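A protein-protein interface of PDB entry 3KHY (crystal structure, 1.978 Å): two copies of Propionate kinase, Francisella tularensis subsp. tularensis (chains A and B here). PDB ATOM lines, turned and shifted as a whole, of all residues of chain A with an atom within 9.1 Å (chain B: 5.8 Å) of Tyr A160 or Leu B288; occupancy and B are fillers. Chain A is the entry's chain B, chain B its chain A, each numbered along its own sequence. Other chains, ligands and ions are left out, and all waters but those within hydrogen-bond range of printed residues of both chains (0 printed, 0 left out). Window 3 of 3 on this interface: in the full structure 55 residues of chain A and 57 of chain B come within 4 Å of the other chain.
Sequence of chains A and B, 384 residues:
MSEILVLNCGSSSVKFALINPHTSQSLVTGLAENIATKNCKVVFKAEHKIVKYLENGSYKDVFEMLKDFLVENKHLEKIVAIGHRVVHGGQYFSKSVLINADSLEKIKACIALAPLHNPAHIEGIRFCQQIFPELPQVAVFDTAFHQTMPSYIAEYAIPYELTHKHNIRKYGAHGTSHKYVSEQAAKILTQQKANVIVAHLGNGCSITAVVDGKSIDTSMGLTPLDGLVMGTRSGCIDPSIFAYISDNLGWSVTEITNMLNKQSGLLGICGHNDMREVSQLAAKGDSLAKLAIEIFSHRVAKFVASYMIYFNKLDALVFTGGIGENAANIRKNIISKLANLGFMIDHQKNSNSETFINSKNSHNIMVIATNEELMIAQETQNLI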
ATOM      1  N   SER A 151     -17.304   6.066 -23.275  1.00  0.00           N
ATOM      2  CA  SER A 151     -15.961   6.186 -23.850  1.00  0.00           C
ATOM      3  C   SER A 151     -15.681   7.572 -24.413  1.00  0.00           C
ATOM      4  O   SER A 151     -14.567   8.093 -24.275  1.00  0.00           O
ATOM      5  CB  SER A 151     -15.756   5.135 -24.950  1.00  0.00           C
ATOM      6  OG  SER A 151     -15.624   3.844 -24.383  1.00  0.00           O
ATOM      7  N   GLU A 155     -12.388   8.680 -22.491  1.00  0.00           N
ATOM      8  CA  GLU A 155     -11.132   8.510 -23.218  1.00  0.00           C
ATOM      9  C   GLU A 155     -10.474   9.834 -23.530  1.00  0.00           C
ATOM     10  O   GLU A 155     -11.154  10.842 -23.746  1.00  0.00           O
ATOM     11  CB  GLU A 155     -11.332   7.707 -24.514  1.00  0.00           C
ATOM     12  CG  GLU A 155     -11.630   6.231 -24.267  1.00  0.00           C
ATOM     13  CD  GLU A 155     -11.743   5.422 -25.534  1.00  0.00           C
ATOM     14  OE1 GLU A 155     -11.377   5.931 -26.638  1.00  0.00           O
ATOM     15  OE2 GLU A 155     -12.212   4.269 -25.416  1.00  0.00           O
ATOM     16  N   TYR A 156      -9.148   9.827 -23.540  1.00  0.00           N
ATOM     17  CA  TYR A 156      -8.374  10.986 -23.967  1.00  0.00           C
ATOM     18  C   TYR A 156      -8.136  10.892 -25.468  1.00  0.00           C
ATOM     19  O   TYR A 156      -8.299   9.817 -26.057  1.00  0.00           O
ATOM     20  CB  TYR A 156      -7.028  11.014 -23.245  1.00  0.00           C
ATOM     21  CG  TYR A 156      -7.151  11.190 -21.743  1.00  0.00           C
ATOM     22  CD1 TYR A 156      -7.706  12.348 -21.202  1.00  0.00           C
ATOM     23  CD2 TYR A 156      -6.712  10.202 -20.866  1.00  0.00           C
ATOM     24  CE1 TYR A 156      -7.813  12.520 -19.818  1.00  0.00           C
ATOM     25  CE2 TYR A 156      -6.816  10.364 -19.486  1.00  0.00           C
ATOM     26  CZ  TYR A 156      -7.366  11.528 -18.970  1.00  0.00           C
ATOM     27  OH  TYR A 156      -7.479  11.694 -17.600  1.00  0.00           O
ATOM     28  N   ALA A 157      -7.748  12.001 -26.095  1.00  0.00           N
ATOM     29  CA  ALA A 157      -7.454  11.961 -27.528  1.00  0.00           C
ATOM     30  C   ALA A 157      -5.981  11.617 -27.749  1.00  0.00           C
ATOM     31  O   ALA A 157      -5.155  12.497 -28.033  1.00  0.00           O
ATOM     32  CB  ALA A 157      -7.806  13.293 -28.189  1.00  0.00           C
ATOM     33  N   ILE A 158      -5.668  10.332 -27.597  1.00  0.00           N
ATOM     34  CA  ILE A 158      -4.306   9.815 -27.693  1.00  0.00           C
ATOM     35  C   ILE A 158      -4.370   8.523 -28.507  1.00  0.00           C
ATOM     36  O   ILE A 158      -5.469   8.050 -28.815  1.00  0.00           O
ATOM     37  CB  ILE A 158      -3.723   9.507 -26.291  1.00  0.00           C
ATOM     38  CG1 ILE A 158      -4.595   8.485 -25.558  1.00  0.00           C
ATOM     39  CG2 ILE A 158      -3.576  10.780 -25.473  1.00  0.00           C
ATOM     40  CD1 ILE A 158      -4.071   8.123 -24.156  1.00  0.00           C
ATOM     41  N   PRO A 159      -3.204   7.953 -28.869  1.00  0.00           N
ATOM     42  CA  PRO A 159      -3.142   6.707 -29.656  1.00  0.00           C
ATOM     43  C   PRO A 159      -4.007   5.567 -29.101  1.00  0.00           C
ATOM     44  O   PRO A 159      -3.979   5.295 -27.910  1.00  0.00           O
ATOM     45  CB  PRO A 159      -1.665   6.319 -29.573  1.00  0.00           C
ATOM     46  CG  PRO A 159      -0.955   7.635 -29.428  1.00  0.00           C
ATOM     47  CD  PRO A 159      -1.860   8.493 -28.586  1.00  0.00           C
ATOM     48  N   TYR A 160      -4.768   4.922 -29.973  1.00  0.00           N
ATOM     49  CA  TYR A 160      -5.571   3.754 -29.617  1.00  0.00           C
ATOM     50  C   TYR A 160      -4.821   2.791 -28.700  1.00  0.00           C
ATOM     51  O   TYR A 160      -5.369   2.307 -27.710  1.00  0.00           O
ATOM     52  CB  TYR A 160      -5.998   3.021 -30.895  1.00  0.00           C
ATOM     53  CG  TYR A 160      -6.915   1.835 -30.679  1.00  0.00           C
ATOM     54  CD1 TYR A 160      -6.406   0.574 -30.396  1.00  0.00           C
ATOM     55  CD2 TYR A 160      -8.289   1.975 -30.779  1.00  0.00           C
ATOM     56  CE1 TYR A 160      -7.254  -0.525 -30.209  1.00  0.00           C
ATOM     57  CE2 TYR A 160      -9.139   0.892 -30.599  1.00  0.00           C
ATOM     58  CZ  TYR A 160      -8.619  -0.351 -30.311  1.00  0.00           C
ATOM     59  OH  TYR A 160      -9.479  -1.420 -30.131  1.00  0.00           O
ATOM     60  N   GLU A 161      -3.566   2.511 -29.021  1.00  0.00           N
ATOM     61  CA  GLU A 161      -2.816   1.513 -28.257  1.00  0.00           C
ATOM     62  C   GLU A 161      -2.567   1.916 -26.800  1.00  0.00           C
ATOM     63  O   GLU A 161      -2.549   1.062 -25.912  1.00  0.00           O
ATOM     64  CB  GLU A 161      -1.488   1.184 -28.941  1.00  0.00           C
ATOM     65  CG  GLU A 161      -0.596   0.290 -28.098  1.00  0.00           C
ATOM     66  CD  GLU A 161       0.468  -0.409 -28.914  1.00  0.00           C
ATOM     67  OE1 GLU A 161       0.101  -1.236 -29.775  1.00  0.00           O
ATOM     68  OE2 GLU A 161       1.666  -0.134 -28.690  1.00  0.00           O
ATOM     69  N   LEU A 162      -2.363   3.208 -26.551  1.00  0.00           N
ATOM     70  CA  LEU A 162      -2.195   3.681 -25.171  1.00  0.00           C
ATOM     71  C   LEU A 162      -3.503   3.573 -24.390  1.00  0.00           C
ATOM     72  O   LEU A 162      -3.532   3.187 -23.213  1.00  0.00           O
ATOM     73  CB  LEU A 162      -1.691   5.126 -25.146  1.00  0.00           C
ATOM     74  CG  LEU A 162      -0.274   5.269 -25.704  1.00  0.00           C
ATOM     75  CD1 LEU A 162       0.193   6.719 -25.636  1.00  0.00           C
ATOM     76  CD2 LEU A 162       0.671   4.351 -24.942  1.00  0.00           C
ATOM     77  N   THR A 163      -4.588   3.927 -25.054  1.00  0.00           N
ATOM     78  CA  THR A 163      -5.915   3.831 -24.455  1.00  0.00           C
ATOM     79  C   THR A 163      -6.259   2.387 -24.097  1.00  0.00           C
ATOM     80  O   THR A 163      -6.717   2.111 -23.000  1.00  0.00           O
ATOM     81  CB  THR A 163      -6.954   4.373 -25.419  1.00  0.00           C
ATOM     82  OG1 THR A 163      -6.707   5.766 -25.622  1.00  0.00           O
ATOM     83  CG2 THR A 163      -8.375   4.172 -24.884  1.00  0.00           C
ATOM     84  N   HIS A 164      -6.020   1.470 -25.024  1.00  0.00           N
ATOM     85  CA  HIS A 164      -6.551   0.119 -24.895  1.00  0.00           C
ATOM     86  C   HIS A 164      -5.548  -0.897 -24.355  1.00  0.00           C
ATOM     87  O   HIS A 164      -5.866  -1.648 -23.437  1.00  0.00           O
ATOM     88  CB  HIS A 164      -7.173  -0.341 -26.219  1.00  0.00           C
ATOM     89  CG  HIS A 164      -8.381   0.449 -26.613  1.00  0.00           C
ATOM     90  ND1 HIS A 164      -9.645   0.157 -26.147  1.00  0.00           N
ATOM     91  CD2 HIS A 164      -8.516   1.537 -27.409  1.00  0.00           C
ATOM     92  CE1 HIS A 164     -10.508   1.025 -26.647  1.00  0.00           C
ATOM     93  NE2 HIS A 164      -9.850   1.873 -27.417  1.00  0.00           N
ATOM     94  N   LYS A 165      -4.332  -0.909 -24.892  1.00  0.00           N
ATOM     95  CA  LYS A 165      -3.330  -1.828 -24.358  1.00  0.00           C
ATOM     96  C   LYS A 165      -2.898  -1.404 -22.953  1.00  0.00           C
ATOM     97  O   LYS A 165      -2.710  -2.242 -22.075  1.00  0.00           O
ATOM     98  CB  LYS A 165      -2.118  -1.934 -25.285  1.00  0.00           C
ATOM     99  CG  LYS A 165      -1.032  -2.875 -24.768  1.00  0.00           C
ATOM    100  CD  LYS A 165       0.101  -3.015 -25.776  1.00  0.00           C
ATOM    101  CE  LYS A 165       1.232  -3.871 -25.221  1.00  0.00           C
ATOM    102  NZ  LYS A 165       2.295  -4.108 -26.237  1.00  0.00           N
ATOM    103  N   HIS A 166      -2.762  -0.101 -22.735  1.00  0.00           N
ATOM    104  CA  HIS A 166      -2.232   0.383 -21.467  1.00  0.00           C
ATOM    105  C   HIS A 166      -3.278   0.997 -20.527  1.00  0.00           C
ATOM    106  O   HIS A 166      -2.939   1.558 -19.485  1.00  0.00           O
ATOM    107  CB  HIS A 166      -1.065   1.332 -21.725  1.00  0.00           C
ATOM    108  CG  HIS A 166       0.058   0.684 -22.472  1.00  0.00           C
ATOM    109  ND1 HIS A 166       0.995  -0.115 -21.857  1.00  0.00           N
ATOM    110  CD2 HIS A 166       0.368   0.682 -23.790  1.00  0.00           C
ATOM    111  CE1 HIS A 166       1.845  -0.568 -22.761  1.00  0.00           C
ATOM    112  NE2 HIS A 166       1.487  -0.099 -23.943  1.00  0.00           N
ATOM    113  N   ASN A 167      -4.546   0.858 -20.897  1.00  0.00           N
ATOM    114  CA  ASN A 167      -5.660   1.270 -20.049  1.00  0.00           C
ATOM    115  C   ASN A 167      -5.621   2.730 -19.600  1.00  0.00           C
ATOM    116  O   ASN A 167      -6.119   3.068 -18.528  1.00  0.00           O
ATOM    117  CB  ASN A 167      -5.759   0.350 -18.834  1.00  0.00           C
ATOM    118  CG  ASN A 167      -5.857  -1.106 -19.224  1.00  0.00           C
ATOM    119  OD1 ASN A 167      -6.773  -1.509 -19.941  1.00  0.00           O
ATOM    120  ND2 ASN A 167      -4.901  -1.904 -18.762  1.00  0.00           N
ATOM    121  N   ILE A 168      -5.029   3.596 -20.414  1.00  0.00           N
ATOM    122  CA  ILE A 168      -4.992   5.015 -20.077  1.00  0.00           C
ATOM    123  C   ILE A 168      -6.299   5.698 -20.482  1.00  0.00           C
ATOM    124  O   ILE A 168      -6.655   5.737 -21.661  1.00  0.00           O
ATOM    125  CB  ILE A 168      -3.800   5.720 -20.733  1.00  0.00           C
ATOM    126  CG1 ILE A 168      -2.487   5.138 -20.189  1.00  0.00           C
ATOM    127  CG2 ILE A 168      -3.884   7.214 -20.504  1.00  0.00           C
ATOM    128  CD1 ILE A 168      -1.245   5.559 -20.982  1.00  0.00           C
ATOM    129  N   ARG A 169      -7.015   6.218 -19.488  1.00  0.00           N
ATOM    130  CA  ARG A 169      -8.274   6.918 -19.706  1.00  0.00           C
ATOM    131  C   ARG A 169      -8.623   7.610 -18.385  1.00  0.00           C
ATOM    132  O   ARG A 169      -7.913   7.446 -17.401  1.00  0.00           O
ATOM    133  CB  ARG A 169      -9.367   5.923 -20.085  1.00  0.00           C
ATOM    134  CG  ARG A 169      -9.809   5.066 -18.900  1.00  0.00           C
ATOM    135  CD  ARG A 169     -10.566   3.817 -19.309  1.00  0.00           C
ATOM    136  NE  ARG A 169     -11.906   4.077 -19.834  1.00  0.00           N
ATOM    137  CZ  ARG A 169     -12.268   3.888 -21.098  1.00  0.00           C
ATOM    138  NH1 ARG A 169     -11.391   3.446 -21.991  1.00  0.00           N
ATOM    139  NH2 ARG A 169     -13.514   4.144 -21.476  1.00  0.00           N
ATOM    140  N   GLY B 268      -4.470  10.046 -33.360  1.00  0.00           N
ATOM    141  CA  GLY B 268      -4.332   9.030 -32.327  1.00  0.00           C
ATOM    142  C   GLY B 268      -5.583   8.188 -32.167  1.00  0.00           C
ATOM    143  O   GLY B 268      -5.513   6.961 -32.073  1.00  0.00           O
ATOM    144  N   ILE B 269      -6.737   8.842 -32.135  1.00  0.00           N
ATOM    145  CA  ILE B 269      -7.999   8.122 -31.940  1.00  0.00           C
ATOM    146  C   ILE B 269      -8.346   7.183 -33.094  1.00  0.00           C
ATOM    147  O   ILE B 269      -8.689   6.019 -32.870  1.00  0.00           O
ATOM    148  CB  ILE B 269      -9.185   9.084 -31.726  1.00  0.00           C
ATOM    149  CG1 ILE B 269      -8.939  10.000 -30.521  1.00  0.00           C
ATOM    150  CG2 ILE B 269     -10.499   8.310 -31.542  1.00  0.00           C
ATOM    151  CD1 ILE B 269      -9.887  11.221 -30.519  1.00  0.00           C
ATOM    152  N   CYS B 270      -8.264   7.672 -34.327  1.00  0.00           N
ATOM    153  CA  CYS B 270      -8.801   6.903 -35.441  1.00  0.00           C
ATOM    154  C   CYS B 270      -7.850   6.662 -36.615  1.00  0.00           C
ATOM    155  O   CYS B 270      -8.229   5.998 -37.583  1.00  0.00           O
ATOM    156  CB  CYS B 270     -10.094   7.543 -35.951  1.00  0.00           C
ATOM    157  SG  CYS B 270      -9.856   9.046 -36.929  1.00  0.00           S
ATOM    158  N   ASP B 286     -17.205   3.799 -40.362  1.00  0.00           N
ATOM    159  CA  ASP B 286     -16.064   3.470 -39.508  1.00  0.00           C
ATOM    160  C   ASP B 286     -16.306   3.933 -38.062  1.00  0.00           C
ATOM    161  O   ASP B 286     -16.390   5.137 -37.798  1.00  0.00           O
ATOM    162  CB  ASP B 286     -14.783   4.095 -40.059  1.00  0.00           C
ATOM    163  CG  ASP B 286     -13.556   3.654 -39.305  1.00  0.00           C
ATOM    164  OD1 ASP B 286     -12.894   2.697 -39.754  1.00  0.00           O
ATOM    165  OD2 ASP B 286     -13.259   4.244 -38.247  1.00  0.00           O
ATOM    166  N   SER B 287     -16.404   2.992 -37.127  1.00  0.00           N
ATOM    167  CA  SER B 287     -16.809   3.352 -35.764  1.00  0.00           C
ATOM    168  C   SER B 287     -15.771   4.172 -34.993  1.00  0.00           C
ATOM    169  O   SER B 287     -16.138   4.960 -34.120  1.00  0.00           O
ATOM    170  CB  SER B 287     -17.221   2.117 -34.947  1.00  0.00           C
ATOM    171  OG  SER B 287     -16.092   1.346 -34.581  1.00  0.00           O
ATOM    172  N   LEU B 288     -14.485   3.979 -35.284  1.00  0.00           N
ATOM    173  CA  LEU B 288     -13.450   4.774 -34.605  1.00  0.00           C
ATOM    174  C   LEU B 288     -13.429   6.214 -35.103  1.00  0.00           C
ATOM    175  O   LEU B 288     -13.162   7.144 -34.328  1.00  0.00           O
ATOM    176  CB  LEU B 288     -12.055   4.150 -34.745  1.00  0.00           C
ATOM    177  CG  LEU B 288     -11.639   3.055 -33.749  1.00  0.00           C
ATOM    178  CD1 LEU B 288     -10.230   2.574 -34.061  1.00  0.00           C
ATOM    179  CD2 LEU B 288     -11.733   3.530 -32.285  1.00  0.00           C
ATOM    180  N   ALA B 289     -13.704   6.410 -36.391  1.00  0.00           N
ATOM    181  CA  ALA B 289     -13.815   7.771 -36.915  1.00  0.00           C
ATOM    182  C   ALA B 289     -15.015   8.455 -36.273  1.00  0.00           C
ATOM    183  O   ALA B 289     -14.967   9.652 -35.936  1.00  0.00           O
ATOM    184  CB  ALA B 289     -13.965   7.760 -38.442  1.00  0.00           C
ATOM    185  N   LYS B 290     -16.101   7.704 -36.123  1.00  0.00           N
ATOM    186  CA  LYS B 290     -17.276   8.222 -35.435  1.00  0.00           C
ATOM    187  C   LYS B 290     -16.937   8.601 -33.992  1.00  0.00           C
ATOM    188  O   LYS B 290     -17.352   9.658 -33.516  1.00  0.00           O
ATOM    189  CB  LYS B 290     -18.439   7.214 -35.469  1.00  0.00           C
ATOM    190  CG  LYS B 290     -19.077   6.999 -36.859  1.00  0.00           C
ATOM    191  CD  LYS B 290     -20.241   5.988 -36.802  1.00  0.00           C
ATOM    192  CE  LYS B 290     -20.782   5.641 -38.199  1.00  0.00           C
ATOM    193  NZ  LYS B 290     -21.395   6.823 -38.858  1.00  0.00           N
ATOM    194  N   LEU B 291     -16.172   7.752 -33.305  1.00  0.00           N
ATOM    195  CA  LEU B 291     -15.775   8.030 -31.917  1.00  0.00           C
ATOM    196  C   LEU B 291     -14.899   9.269 -31.827  1.00  0.00           C
ATOM    197  O   LEU B 291     -15.025  10.065 -30.892  1.00  0.00           O
ATOM    198  CB  LEU B 291     -15.026   6.837 -31.306  1.00  0.00           C
ATOM    199  CG  LEU B 291     -14.560   7.035 -29.858  1.00  0.00           C
ATOM    200  CD1 LEU B 291     -15.752   7.293 -28.908  1.00  0.00           C
ATOM    201  CD2 LEU B 291     -13.718   5.852 -29.370  1.00  0.00           C
ATOM    202  N   ALA B 292     -13.990   9.417 -32.786  1.00  0.00           N
ATOM    203  CA  ALA B 292     -13.108  10.580 -32.821  1.00  0.00           C
ATOM    204  C   ALA B 292     -13.941  11.857 -32.935  1.00  0.00           C
ATOM    205  O   ALA B 292     -13.650  12.863 -32.286  1.00  0.00           O
ATOM    206  CB  ALA B 292     -12.126  10.474 -33.993  1.00  0.00           C
ATOM    207  N   ILE B 293     -14.980  11.812 -33.763  1.00  0.00           N
ATOM    208  CA  ILE B 293     -15.863  12.965 -33.930  1.00  0.00           C
ATOM    209  C   ILE B 293     -16.674  13.247 -32.662  1.00  0.00           C
ATOM    210  O   ILE B 293     -16.869  14.405 -32.306  1.00  0.00           O
ATOM    211  CB  ILE B 293     -16.788  12.793 -35.161  1.00  0.00           C
ATOM    212  CG1 ILE B 293     -15.975  12.969 -36.452  1.00  0.00           C
ATOM    213  CG2 ILE B 293     -17.944  13.797 -35.136  1.00  0.00           C
ATOM    214  CD1 ILE B 293     -16.749  12.602 -37.722  1.00  0.00           C
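The backbone NH (N) of Tyr A160 is in hydrogen-bond range of the backbone carbonyl oxygen (O) of Gly B268 (3.0 Å). O of Gly B268 sits close to O of Ile A158 (3.4 Å).
OD2 of Asp B286 lies within hydrogen-bond range of N of Leu B288 (3.2 Å). OE2 of Glu A155 lies within salt-bridge range of NH1 of Arg A169, 3.6 Å away.
Among the printed residues, merely in contact across the chains: Pro A159 with Gly B268, Glu A155 with Leu B291, Ile A158 with Ile B269, Ala A157 with Ile B269 and Tyr A160 with Leu B288.
Of chain B, only Gly B268 and Leu B288 come within 4 Å of Tyr A160. Leu B288 touches just one residue of chain A: Tyr A160. No residue of chain A comes within 4 Å of Ser B287. No residue of chain A comes within 4 Å of Ala B289. Printed residues of chain B within 4 Å of Pro A159: Gly B268 (3.4 Å). Printed residues of chain B within 4 Å of Ala A157: Ile B269 (3.7 Å). Printed residues of chain A within 4 Å of Ile B269: Ala A157 and Ile A158. Of the printed residues of chain A, Gly B268 touches Ile A158, Pro A159 and Tyr A160. Of the printed residues of chain B, Ile A158 touches Gly B268 (3.4 Å) and Ile B269 (3.6 Å). Ser A151 touches none of the printed residues of chain B. Asn A167 touches none of the printed residues of chain B. The nearest residue of chain B that does not touch Tyr A160 is Ile B269 (4.5 Å). The nearest printed residue of chain B that does not touch Ala A157 is Gly B268 (5.5 Å).
Printed residues of chain B that touch a printed residue of chain A: Gly B268, Ile B269, Leu B288 and Leu B291. Hydrophobic or aromatic side chains of chain B that line the printed part of chain A: Ile B269, Leu B288 and Leu B291. Of the 16 printed residues of chain A, 5 touch a printed residue of chain B. Among the printed residues, no Asp or Glu carboxylate lies within 4 Å of a Lys or Arg side-chain nitrogen of the other chain.
No position is printed for both chains.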
